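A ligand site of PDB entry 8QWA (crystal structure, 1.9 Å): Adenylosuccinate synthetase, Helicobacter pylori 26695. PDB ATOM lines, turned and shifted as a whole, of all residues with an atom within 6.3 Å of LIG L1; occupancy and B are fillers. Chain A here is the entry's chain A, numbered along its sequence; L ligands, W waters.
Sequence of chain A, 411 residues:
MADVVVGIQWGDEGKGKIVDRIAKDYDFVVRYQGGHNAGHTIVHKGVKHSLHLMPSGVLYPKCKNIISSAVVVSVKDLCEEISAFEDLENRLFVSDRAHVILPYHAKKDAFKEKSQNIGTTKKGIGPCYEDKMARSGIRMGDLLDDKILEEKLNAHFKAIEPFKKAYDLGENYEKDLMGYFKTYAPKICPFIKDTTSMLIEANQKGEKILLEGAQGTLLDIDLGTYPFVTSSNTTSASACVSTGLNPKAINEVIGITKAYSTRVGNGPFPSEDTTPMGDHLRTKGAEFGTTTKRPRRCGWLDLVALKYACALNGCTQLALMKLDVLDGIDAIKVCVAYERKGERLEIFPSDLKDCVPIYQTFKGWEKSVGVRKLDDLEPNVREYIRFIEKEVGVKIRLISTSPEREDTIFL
O of Asp 12 sits at hydrogen-bond distance from NZ of Lys 322 (3.2 Å).
O of Gln 215 is in hydrogen-bond range of NZ of Lys 15, 3.1 Å away.
The side-chain carboxylate (OE2) of Glu 13 is in hydrogen-bond range of the backbone NH (N) of Gly 11 (2.9 Å).
OD2 of Asp 12 is in salt-bridge range of NE of Arg 296, 2.7 Å away.
The side-chain amino group (NZ) of Lys 258 sits at hydrogen-bond distance from the backbone carbonyl oxygen (O) of Asp 12 (2.8 Å).
OG1 of Thr 41 is in hydrogen-bond range of O of Gly 39.
O of Ala 286 lies within hydrogen-bond range of N of Arg 296 (2.9 Å).
The guanidinium group (NH1) of Arg 296 lies within hydrogen-bond range of the backbone carbonyl oxygen (O) of Arg 294 (2.7 Å).
C5 of LIG L1 is covalently linked to NZ of Lys 322, at 1.3 Å.
O4 of LIG L1 is in hydrogen-bond range of N of Lys 15 (2.9 Å).
O4 of LIG L1 is in salt-bridge range of NZ of Lys 15.
An oxygen (O3) of LIG L1 sits at hydrogen-bond distance from the backbone NH of Gly 16 (2.9 Å).
The backbone NH (N) of Gly 14 is in hydrogen-bond range of an oxygen (O4) of LIG L1 (3.0 Å).
N of Glu 13 is in hydrogen-bond range of O4 of LIG L1.
The side-chain carboxylate (OD1) of Asp 12 is in hydrogen-bond range of a nitrogen (N3) of LG2 L2, 3.0 Å away.
NE2 of Gln 215 lies within hydrogen-bond range of N2 of LG2 L2 (3.2 Å).
An oxygen (O7) of LG2 L2 lies within hydrogen-bond range of the guanidinium group (NH2) of Arg 294 (2.8 Å).
O of Asp 12 touches C5 of LIG L1 (3.3 Å).
O of Gly 39 touches O5 of LIG L1 (3.9 Å).
His 40 touches LIG L1.
Thr 41 touches LIG L1.
Lys 258 touches LIG L1.
Arg 296 touches LIG L1.
Hydrophobic or aromatic side chains within 4 Å of LIG L1: His 40.
11 residues have an atom within 4 Å of LIG L1: Asp 12, Glu 13, Gly 14, Lys 15, Gly 16, Gly 39, His 40, Thr 41, Lys 258, Arg 296 and Lys 322.
Water W4 lies within hydrogen-bond range of O1 of LIG L1 (2.6 Å), O of Gly 285 (2.7 Å), OH of Tyr 260 (2.8 Å) and NZ of Lys 258 (3.1 Å).
Water W2 lies within hydrogen-bond range of O3 of LIG L1 (2.6 Å), O of Thr 41 (2.9 Å), N of Lys 17 (3.0 Å) and N of Gly 16 (3.4 Å).
Water W3 lies within hydrogen-bond range of an oxygen (O5) of LIG L1 (2.7 Å), the side-chain amino group of Lys 15 (2.8 Å), the backbone NH of Asp 12 (2.9 Å) and an oxygen (O8) of LG2 L2 (3.0 Å).
Water W1 lies within hydrogen-bond range of the side-chain carboxylate (OD1) of Asp 12 (2.8 Å) and an oxygen (O5) of LIG L1 (2.9 Å).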
ATOM      1  N   GLY A  11      17.433  31.022 -25.514  1.00  0.00           N
ATOM      2  CA  GLY A  11      17.437  30.452 -24.185  1.00  0.00           C
ATOM      3  C   GLY A  11      18.737  29.696 -23.882  1.00  0.00           C
ATOM      4  O   GLY A  11      19.604  29.581 -24.732  1.00  0.00           O
ATOM      5  N   ASP A  12      18.883  29.273 -22.619  1.00  0.00           N
ATOM      6  CA  ASP A  12      20.010  28.467 -22.197  1.00  0.00           C
ATOM      7  C   ASP A  12      21.336  29.209 -22.347  1.00  0.00           C
ATOM      8  O   ASP A  12      22.360  28.564 -22.572  1.00  0.00           O
ATOM      9  CB  ASP A  12      20.062  27.120 -22.928  1.00  0.00           C
ATOM     10  CG  ASP A  12      18.744  26.350 -22.919  1.00  0.00           C
ATOM     11  OD1 ASP A  12      18.029  26.479 -21.892  1.00  0.00           O
ATOM     12  OD2 ASP A  12      18.416  25.681 -23.937  1.00  0.00           O
ATOM     13  N   GLU A  13      21.311  30.530 -22.253  1.00  0.00           N
ATOM     14  CA  GLU A  13      22.524  31.318 -22.524  1.00  0.00           C
ATOM     15  C   GLU A  13      23.397  31.420 -21.276  1.00  0.00           C
ATOM     16  O   GLU A  13      24.598  31.732 -21.382  1.00  0.00           O
ATOM     17  CB  GLU A  13      22.240  32.743 -22.994  1.00  0.00           C
ATOM     18  CG  GLU A  13      21.357  32.866 -24.231  1.00  0.00           C
ATOM     19  CD  GLU A  13      19.855  32.956 -24.055  1.00  0.00           C
ATOM     20  OE1 GLU A  13      19.347  32.621 -22.943  1.00  0.00           O
ATOM     21  OE2 GLU A  13      19.178  33.340 -25.039  1.00  0.00           O
ATOM     22  N   GLY A  14      22.792  31.182 -20.094  1.00  0.00           N
ATOM     23  CA  GLY A  14      23.464  31.319 -18.814  1.00  0.00           C
ATOM     24  C   GLY A  14      22.965  32.496 -17.974  1.00  0.00           C
ATOM     25  O   GLY A  14      23.707  33.096 -17.197  1.00  0.00           O
ATOM     26  N   LYS A  15      21.665  32.796 -18.073  1.00  0.00           N
ATOM     27  CA  LYS A  15      21.047  33.896 -17.383  1.00  0.00           C
ATOM     28  C   LYS A  15      21.040  33.701 -15.871  1.00  0.00           C
ATOM     29  O   LYS A  15      21.257  34.658 -15.081  1.00  0.00           O
ATOM     30  CB  LYS A  15      19.598  34.089 -17.854  1.00  0.00           C
ATOM     31  CG  LYS A  15      19.505  34.516 -19.279  1.00  0.00           C
ATOM     32  CD  LYS A  15      18.117  34.535 -19.880  1.00  0.00           C
ATOM     33  CE  LYS A  15      17.307  33.275 -19.837  1.00  0.00           C
ATOM     34  NZ  LYS A  15      17.922  32.103 -20.497  1.00  0.00           N
ATOM     35  N   GLY A  16      20.705  32.491 -15.462  1.00  0.00           N
ATOM     36  CA  GLY A  16      20.625  32.188 -14.024  1.00  0.00           C
ATOM     37  C   GLY A  16      21.966  32.460 -13.323  1.00  0.00           C
ATOM     38  O   GLY A  16      22.030  33.078 -12.243  1.00  0.00           O
ATOM     39  N   LYS A  17      23.044  32.057 -13.976  1.00  0.00           N
ATOM     40  CA  LYS A  17      24.361  32.266 -13.439  1.00  0.00           C
ATOM     41  C   LYS A  17      24.631  33.748 -13.299  1.00  0.00           C
ATOM     42  O   LYS A  17      25.100  34.178 -12.266  1.00  0.00           O
ATOM     43  CB  LYS A  17      25.473  31.586 -14.262  1.00  0.00           C
ATOM     44  CG  LYS A  17      26.815  32.058 -13.784  1.00  0.00           C
ATOM     45  CD  LYS A  17      28.071  31.404 -14.335  1.00  0.00           C
ATOM     46  CE  LYS A  17      29.217  32.314 -13.990  1.00  0.00           C
ATOM     47  NZ  LYS A  17      30.523  31.748 -14.235  1.00  0.00           N
ATOM     48  N   ALA A  38      11.312  27.682 -17.980  1.00  0.00           N
ATOM     49  CA  ALA A  38      12.676  28.089 -17.657  1.00  0.00           C
ATOM     50  C   ALA A  38      13.365  27.049 -16.770  1.00  0.00           C
ATOM     51  O   ALA A  38      12.659  26.377 -16.018  1.00  0.00           O
ATOM     52  CB  ALA A  38      12.631  29.434 -16.948  1.00  0.00           C
ATOM     53  N   GLY A  39      14.718  27.020 -16.807  1.00  0.00           N
ATOM     54  CA  GLY A  39      15.566  26.197 -15.936  1.00  0.00           C
ATOM     55  C   GLY A  39      16.857  26.927 -15.493  1.00  0.00           C
ATOM     56  O   GLY A  39      17.926  26.401 -15.643  1.00  0.00           O
ATOM     57  N   HIS A  40      16.760  28.167 -14.950  1.00  0.00           N
ATOM     58  CA  HIS A  40      17.916  29.006 -14.632  1.00  0.00           C
ATOM     59  C   HIS A  40      18.796  28.309 -13.607  1.00  0.00           C
ATOM     60  O   HIS A  40      18.302  27.878 -12.547  1.00  0.00           O
ATOM     61  CB  HIS A  40      17.453  30.354 -14.082  1.00  0.00           C
ATOM     62  CG  HIS A  40      16.760  31.132 -15.175  1.00  0.00           C
ATOM     63  ND1 HIS A  40      16.308  32.447 -15.056  1.00  0.00           N
ATOM     64  CD2 HIS A  40      16.400  30.718 -16.466  1.00  0.00           C
ATOM     65  CE1 HIS A  40      15.733  32.805 -16.204  1.00  0.00           C
ATOM     66  NE2 HIS A  40      15.795  31.766 -17.066  1.00  0.00           N
ATOM     67  N   THR A  41      20.054  28.111 -13.960  1.00  0.00           N
ATOM     68  CA  THR A  41      20.882  27.198 -13.158  1.00  0.00           C
ATOM     69  C   THR A  41      22.069  27.930 -12.555  1.00  0.00           C
ATOM     70  O   THR A  41      22.811  28.677 -13.234  1.00  0.00           O
ATOM     71  CB  THR A  41      21.287  25.936 -13.911  1.00  0.00           C
ATOM     72  OG1 THR A  41      20.007  25.548 -14.406  1.00  0.00           O
ATOM     73  CG2 THR A  41      21.863  24.879 -12.983  1.00  0.00           C
ATOM     74  N   GLN A 215      13.703  32.420 -21.161  1.00  0.00           N
ATOM     75  CA  GLN A 215      13.837  32.069 -22.570  1.00  0.00           C
ATOM     76  C   GLN A 215      14.888  32.949 -23.193  1.00  0.00           C
ATOM     77  O   GLN A 215      15.961  33.121 -22.612  1.00  0.00           O
ATOM     78  CB  GLN A 215      12.478  32.111 -23.265  1.00  0.00           C
ATOM     79  CG  GLN A 215      11.558  30.990 -22.808  1.00  0.00           C
ATOM     80  CD  GLN A 215      10.899  31.246 -21.489  1.00  0.00           C
ATOM     81  OE1 GLN A 215      10.291  32.291 -21.248  1.00  0.00           O
ATOM     82  NE2 GLN A 215      11.021  30.277 -20.600  1.00  0.00           N
ATOM     83  N   ILE A 256      22.902  38.306 -22.481  1.00  0.00           N
ATOM     84  CA  ILE A 256      23.566  37.062 -22.136  1.00  0.00           C
ATOM     85  C   ILE A 256      23.665  36.231 -23.397  1.00  0.00           C
ATOM     86  O   ILE A 256      22.633  35.896 -24.020  1.00  0.00           O
ATOM     87  CB  ILE A 256      22.834  36.276 -21.032  1.00  0.00           C
ATOM     88  CG1 ILE A 256      22.430  37.159 -19.880  1.00  0.00           C
ATOM     89  CG2 ILE A 256      23.729  35.131 -20.541  1.00  0.00           C
ATOM     90  CD1 ILE A 256      23.548  37.995 -19.283  1.00  0.00           C
ATOM     91  N   LYS A 258      25.753  33.030 -25.212  1.00  0.00           N
ATOM     92  CA  LYS A 258      26.669  31.909 -25.198  1.00  0.00           C
ATOM     93  C   LYS A 258      27.721  32.122 -26.295  1.00  0.00           C
ATOM     94  O   LYS A 258      27.474  32.767 -27.307  1.00  0.00           O
ATOM     95  CB  LYS A 258      25.791  30.664 -25.308  1.00  0.00           C
ATOM     96  CG  LYS A 258      26.337  29.440 -24.714  1.00  0.00           C
ATOM     97  CD  LYS A 258      25.339  28.343 -24.300  1.00  0.00           C
ATOM     98  CE  LYS A 258      24.330  28.019 -25.352  1.00  0.00           C
ATOM     99  NZ  LYS A 258      23.234  27.192 -24.894  1.00  0.00           N
ATOM    100  N   TYR A 260      28.757  29.922 -28.254  1.00  0.00           N
ATOM    101  CA  TYR A 260      28.220  29.165 -29.379  1.00  0.00           C
ATOM    102  C   TYR A 260      26.696  29.247 -29.256  1.00  0.00           C
ATOM    103  O   TYR A 260      26.193  29.809 -28.276  1.00  0.00           O
ATOM    104  CB  TYR A 260      28.762  27.720 -29.344  1.00  0.00           C
ATOM    105  CG  TYR A 260      28.389  26.982 -28.067  1.00  0.00           C
ATOM    106  CD1 TYR A 260      29.107  27.186 -26.902  1.00  0.00           C
ATOM    107  CD2 TYR A 260      27.272  26.154 -27.999  1.00  0.00           C
ATOM    108  CE1 TYR A 260      28.732  26.613 -25.689  1.00  0.00           C
ATOM    109  CE2 TYR A 260      26.895  25.561 -26.804  1.00  0.00           C
ATOM    110  CZ  TYR A 260      27.630  25.806 -25.646  1.00  0.00           C
ATOM    111  OH  TYR A 260      27.329  25.276 -24.434  1.00  0.00           O
ATOM    112  N   THR A 262      22.658  27.408 -29.185  1.00  0.00           N
ATOM    113  CA  THR A 262      21.755  26.247 -29.151  1.00  0.00           C
ATOM    114  C   THR A 262      20.303  26.641 -29.421  1.00  0.00           C
ATOM    115  O   THR A 262      19.901  27.797 -29.220  1.00  0.00           O
ATOM    116  CB  THR A 262      21.806  25.583 -27.772  1.00  0.00           C
ATOM    117  OG1 THR A 262      21.478  26.523 -26.749  1.00  0.00           O
ATOM    118  CG2 THR A 262      23.197  25.072 -27.469  1.00  0.00           C
ATOM    119  N   GLY A 285      28.182  20.591 -24.947  1.00  0.00           N
ATOM    120  CA  GLY A 285      27.157  21.641 -24.880  1.00  0.00           C
ATOM    121  C   GLY A 285      25.691  21.221 -25.168  1.00  0.00           C
ATOM    122  O   GLY A 285      24.765  22.041 -25.015  1.00  0.00           O
ATOM    123  N   ALA A 286      25.430  19.979 -25.610  1.00  0.00           N
ATOM    124  CA  ALA A 286      24.045  19.563 -25.879  1.00  0.00           C
ATOM    125  C   ALA A 286      23.269  19.394 -24.564  1.00  0.00           C
ATOM    126  O   ALA A 286      22.050  19.570 -24.558  1.00  0.00           O
ATOM    127  CB  ALA A 286      24.020  18.281 -26.710  1.00  0.00           C
ATOM    128  N   GLU A 287      23.971  19.067 -23.454  1.00  0.00           N
ATOM    129  CA  GLU A 287      23.376  18.625 -22.186  1.00  0.00           C
ATOM    130  C   GLU A 287      23.747  19.574 -21.021  1.00  0.00           C
ATOM    131  O   GLU A 287      24.972  19.867 -20.899  1.00  0.00           O
ATOM    132  CB  GLU A 287      23.822  17.167 -21.964  1.00  0.00           C
ATOM    133  CG  GLU A 287      25.299  16.984 -21.583  1.00  0.00           C
ATOM    134  CD  GLU A 287      26.469  17.136 -22.576  1.00  0.00           C
ATOM    135  OE1 GLU A 287      27.551  16.733 -22.077  1.00  0.00           O
ATOM    136  OE2 GLU A 287      26.437  17.613 -23.751  1.00  0.00           O
ATOM    137  N   ARG A 294      15.918  17.582 -22.638  1.00  0.00           N
ATOM    138  CA  ARG A 294      16.002  17.346 -24.058  1.00  0.00           C
ATOM    139  C   ARG A 294      17.344  17.864 -24.536  1.00  0.00           C
ATOM    140  O   ARG A 294      17.794  18.924 -24.096  1.00  0.00           O
ATOM    141  CB  ARG A 294      14.887  18.122 -24.751  1.00  0.00           C
ATOM    142  CG  ARG A 294      13.460  17.664 -24.497  1.00  0.00           C
ATOM    143  CD  ARG A 294      12.453  18.557 -25.227  1.00  0.00           C
ATOM    144  NE  ARG A 294      12.435  19.904 -24.631  1.00  0.00           N
ATOM    145  CZ  ARG A 294      12.022  20.995 -25.278  1.00  0.00           C
ATOM    146  NH1 ARG A 294      11.547  20.917 -26.513  1.00  0.00           N
ATOM    147  NH2 ARG A 294      12.089  22.169 -24.672  1.00  0.00           N
ATOM    148  N   ARG A 296      20.135  19.743 -26.672  1.00  0.00           N
ATOM    149  CA  ARG A 296      20.059  20.930 -27.505  1.00  0.00           C
ATOM    150  C   ARG A 296      20.713  20.664 -28.876  1.00  0.00           C
ATOM    151  O   ARG A 296      21.755  20.015 -28.978  1.00  0.00           O
ATOM    152  CB  ARG A 296      20.784  22.091 -26.793  1.00  0.00           C
ATOM    153  CG  ARG A 296      19.980  22.883 -25.759  1.00  0.00           C
ATOM    154  CD  ARG A 296      19.252  22.074 -24.694  1.00  0.00           C
ATOM    155  NE  ARG A 296      18.466  23.009 -23.871  1.00  0.00           N
ATOM    156  CZ  ARG A 296      17.558  22.609 -22.995  1.00  0.00           C
ATOM    157  NH1 ARG A 296      17.254  21.310 -22.909  1.00  0.00           N
ATOM    158  NH2 ARG A 296      16.925  23.491 -22.244  1.00  0.00           N
ATOM    159  N   LYS A 322      30.055  30.331 -21.168  1.00  0.00           N
ATOM    160  CA  LYS A 322      30.352  28.933 -21.448  1.00  0.00           C
ATOM    161  C   LYS A 322      31.562  28.752 -22.341  1.00  0.00           C
ATOM    162  O   LYS A 322      31.606  27.866 -23.205  1.00  0.00           O
ATOM    163  CB  LYS A 322      29.151  28.143 -21.983  1.00  0.00           C
ATOM    164  CG  LYS A 322      27.930  28.478 -21.128  1.00  0.00           C
ATOM    165  CD  LYS A 322      26.822  27.461 -21.102  1.00  0.00           C
ATOM    166  CE  LYS A 322      25.630  28.085 -20.314  1.00  0.00           C
ATOM    167  NZ  LYS A 322      24.521  27.211 -20.608  1.00  0.00           N
HETATM  168  N1  LIG L   1      20.580  24.192 -20.399  1.00  0.00           N
HETATM  169  C1  LIG L   1      21.691  24.161 -21.141  1.00  0.00           C
HETATM  170  C2  LIG L   1      21.867  23.063 -22.129  1.00  0.00           C
HETATM  171  C3  LIG L   1      22.658  25.133 -20.960  1.00  0.00           C
HETATM  172  O1  LIG L   1      23.800  25.179 -21.686  1.00  0.00           O
HETATM  173  C4  LIG L   1      22.476  26.162 -19.999  1.00  0.00           C
HETATM  174  C5  LIG L   1      23.506  27.176 -19.829  1.00  0.00           C
HETATM  175  C6  LIG L   1      21.315  26.164 -19.230  1.00  0.00           C
HETATM  176  C7  LIG L   1      20.404  25.167 -19.462  1.00  0.00           C
HETATM  177  C8  LIG L   1      21.043  27.247 -18.214  1.00  0.00           C
HETATM  178  O2  LIG L   1      20.895  28.596 -18.827  1.00  0.00           O
HETATM  179  P1  LIG L   1      19.860  29.738 -18.355  1.00  0.00           P
HETATM  180  O3  LIG L   1      20.320  29.997 -16.958  1.00  0.00           O
HETATM  181  O4  LIG L   1      19.921  30.906 -19.342  1.00  0.00           O
HETATM  182  O5  LIG L   1      18.464  29.081 -18.416  1.00  0.00           O
HETATM  183  P1  LG2 L   2       7.018  26.730 -24.449  1.00  0.00           P
HETATM  184  O1  LG2 L   2       6.956  25.524 -23.527  1.00  0.00           O
HETATM  185  O2  LG2 L   2       7.620  27.963 -23.810  1.00  0.00           O
HETATM  186  O3  LG2 L   2       5.698  27.013 -25.156  1.00  0.00           O
HETATM  187  O4  LG2 L   2       8.106  26.264 -25.573  1.00  0.00           O
HETATM  188  C1  LG2 L   2       8.204  27.049 -26.814  1.00  0.00           C
HETATM  189  C2  LG2 L   2       9.635  27.100 -27.322  1.00  0.00           C
HETATM  190  O5  LG2 L   2      10.500  27.778 -26.365  1.00  0.00           O
HETATM  191  C3  LG2 L   2      10.327  25.765 -27.582  1.00  0.00           C
HETATM  192  O6  LG2 L   2      11.242  25.851 -28.659  1.00  0.00           O
HETATM  193  C4  LG2 L   2      10.983  25.467 -26.239  1.00  0.00           C
HETATM  194  O7  LG2 L   2      11.959  24.427 -26.336  1.00  0.00           O
HETATM  195  C5  LG2 L   2      11.502  26.882 -25.946  1.00  0.00           C
HETATM  196  N1  LG2 L   2      11.800  27.150 -24.556  1.00  0.00           N
HETATM  197  C6  LG2 L   2      10.973  27.471 -23.515  1.00  0.00           C
HETATM  198  N2  LG2 L   2      11.616  27.713 -22.398  1.00  0.00           N
HETATM  199  C7  LG2 L   2      12.957  27.489 -22.730  1.00  0.00           C
HETATM  200  C8  LG2 L   2      14.137  27.586 -21.941  1.00  0.00           C
HETATM  201  O8  LG2 L   2      14.261  27.894 -20.755  1.00  0.00           O
HETATM  202  N3  LG2 L   2      15.267  27.246 -22.716  1.00  0.00           N
HETATM  203  C9  LG2 L   2      15.265  26.956 -24.042  1.00  0.00           C
HETATM  204  N4  LG2 L   2      14.179  26.873 -24.781  1.00  0.00           N
HETATM  205  C10 LG2 L   2      13.069  27.168 -24.063  1.00  0.00           C
HETATM  206  O   HOH W   1      17.310  26.594 -19.206  1.00  0.00           O
HETATM  207  O   HOH W   2      22.737  29.756 -15.900  1.00  0.00           O
HETATM  208  O   HOH W   3      16.813  29.483 -20.538  1.00  0.00           O
HETATM  209  O   HOH W   4      24.699  24.541 -24.040  1.00  0.00           O
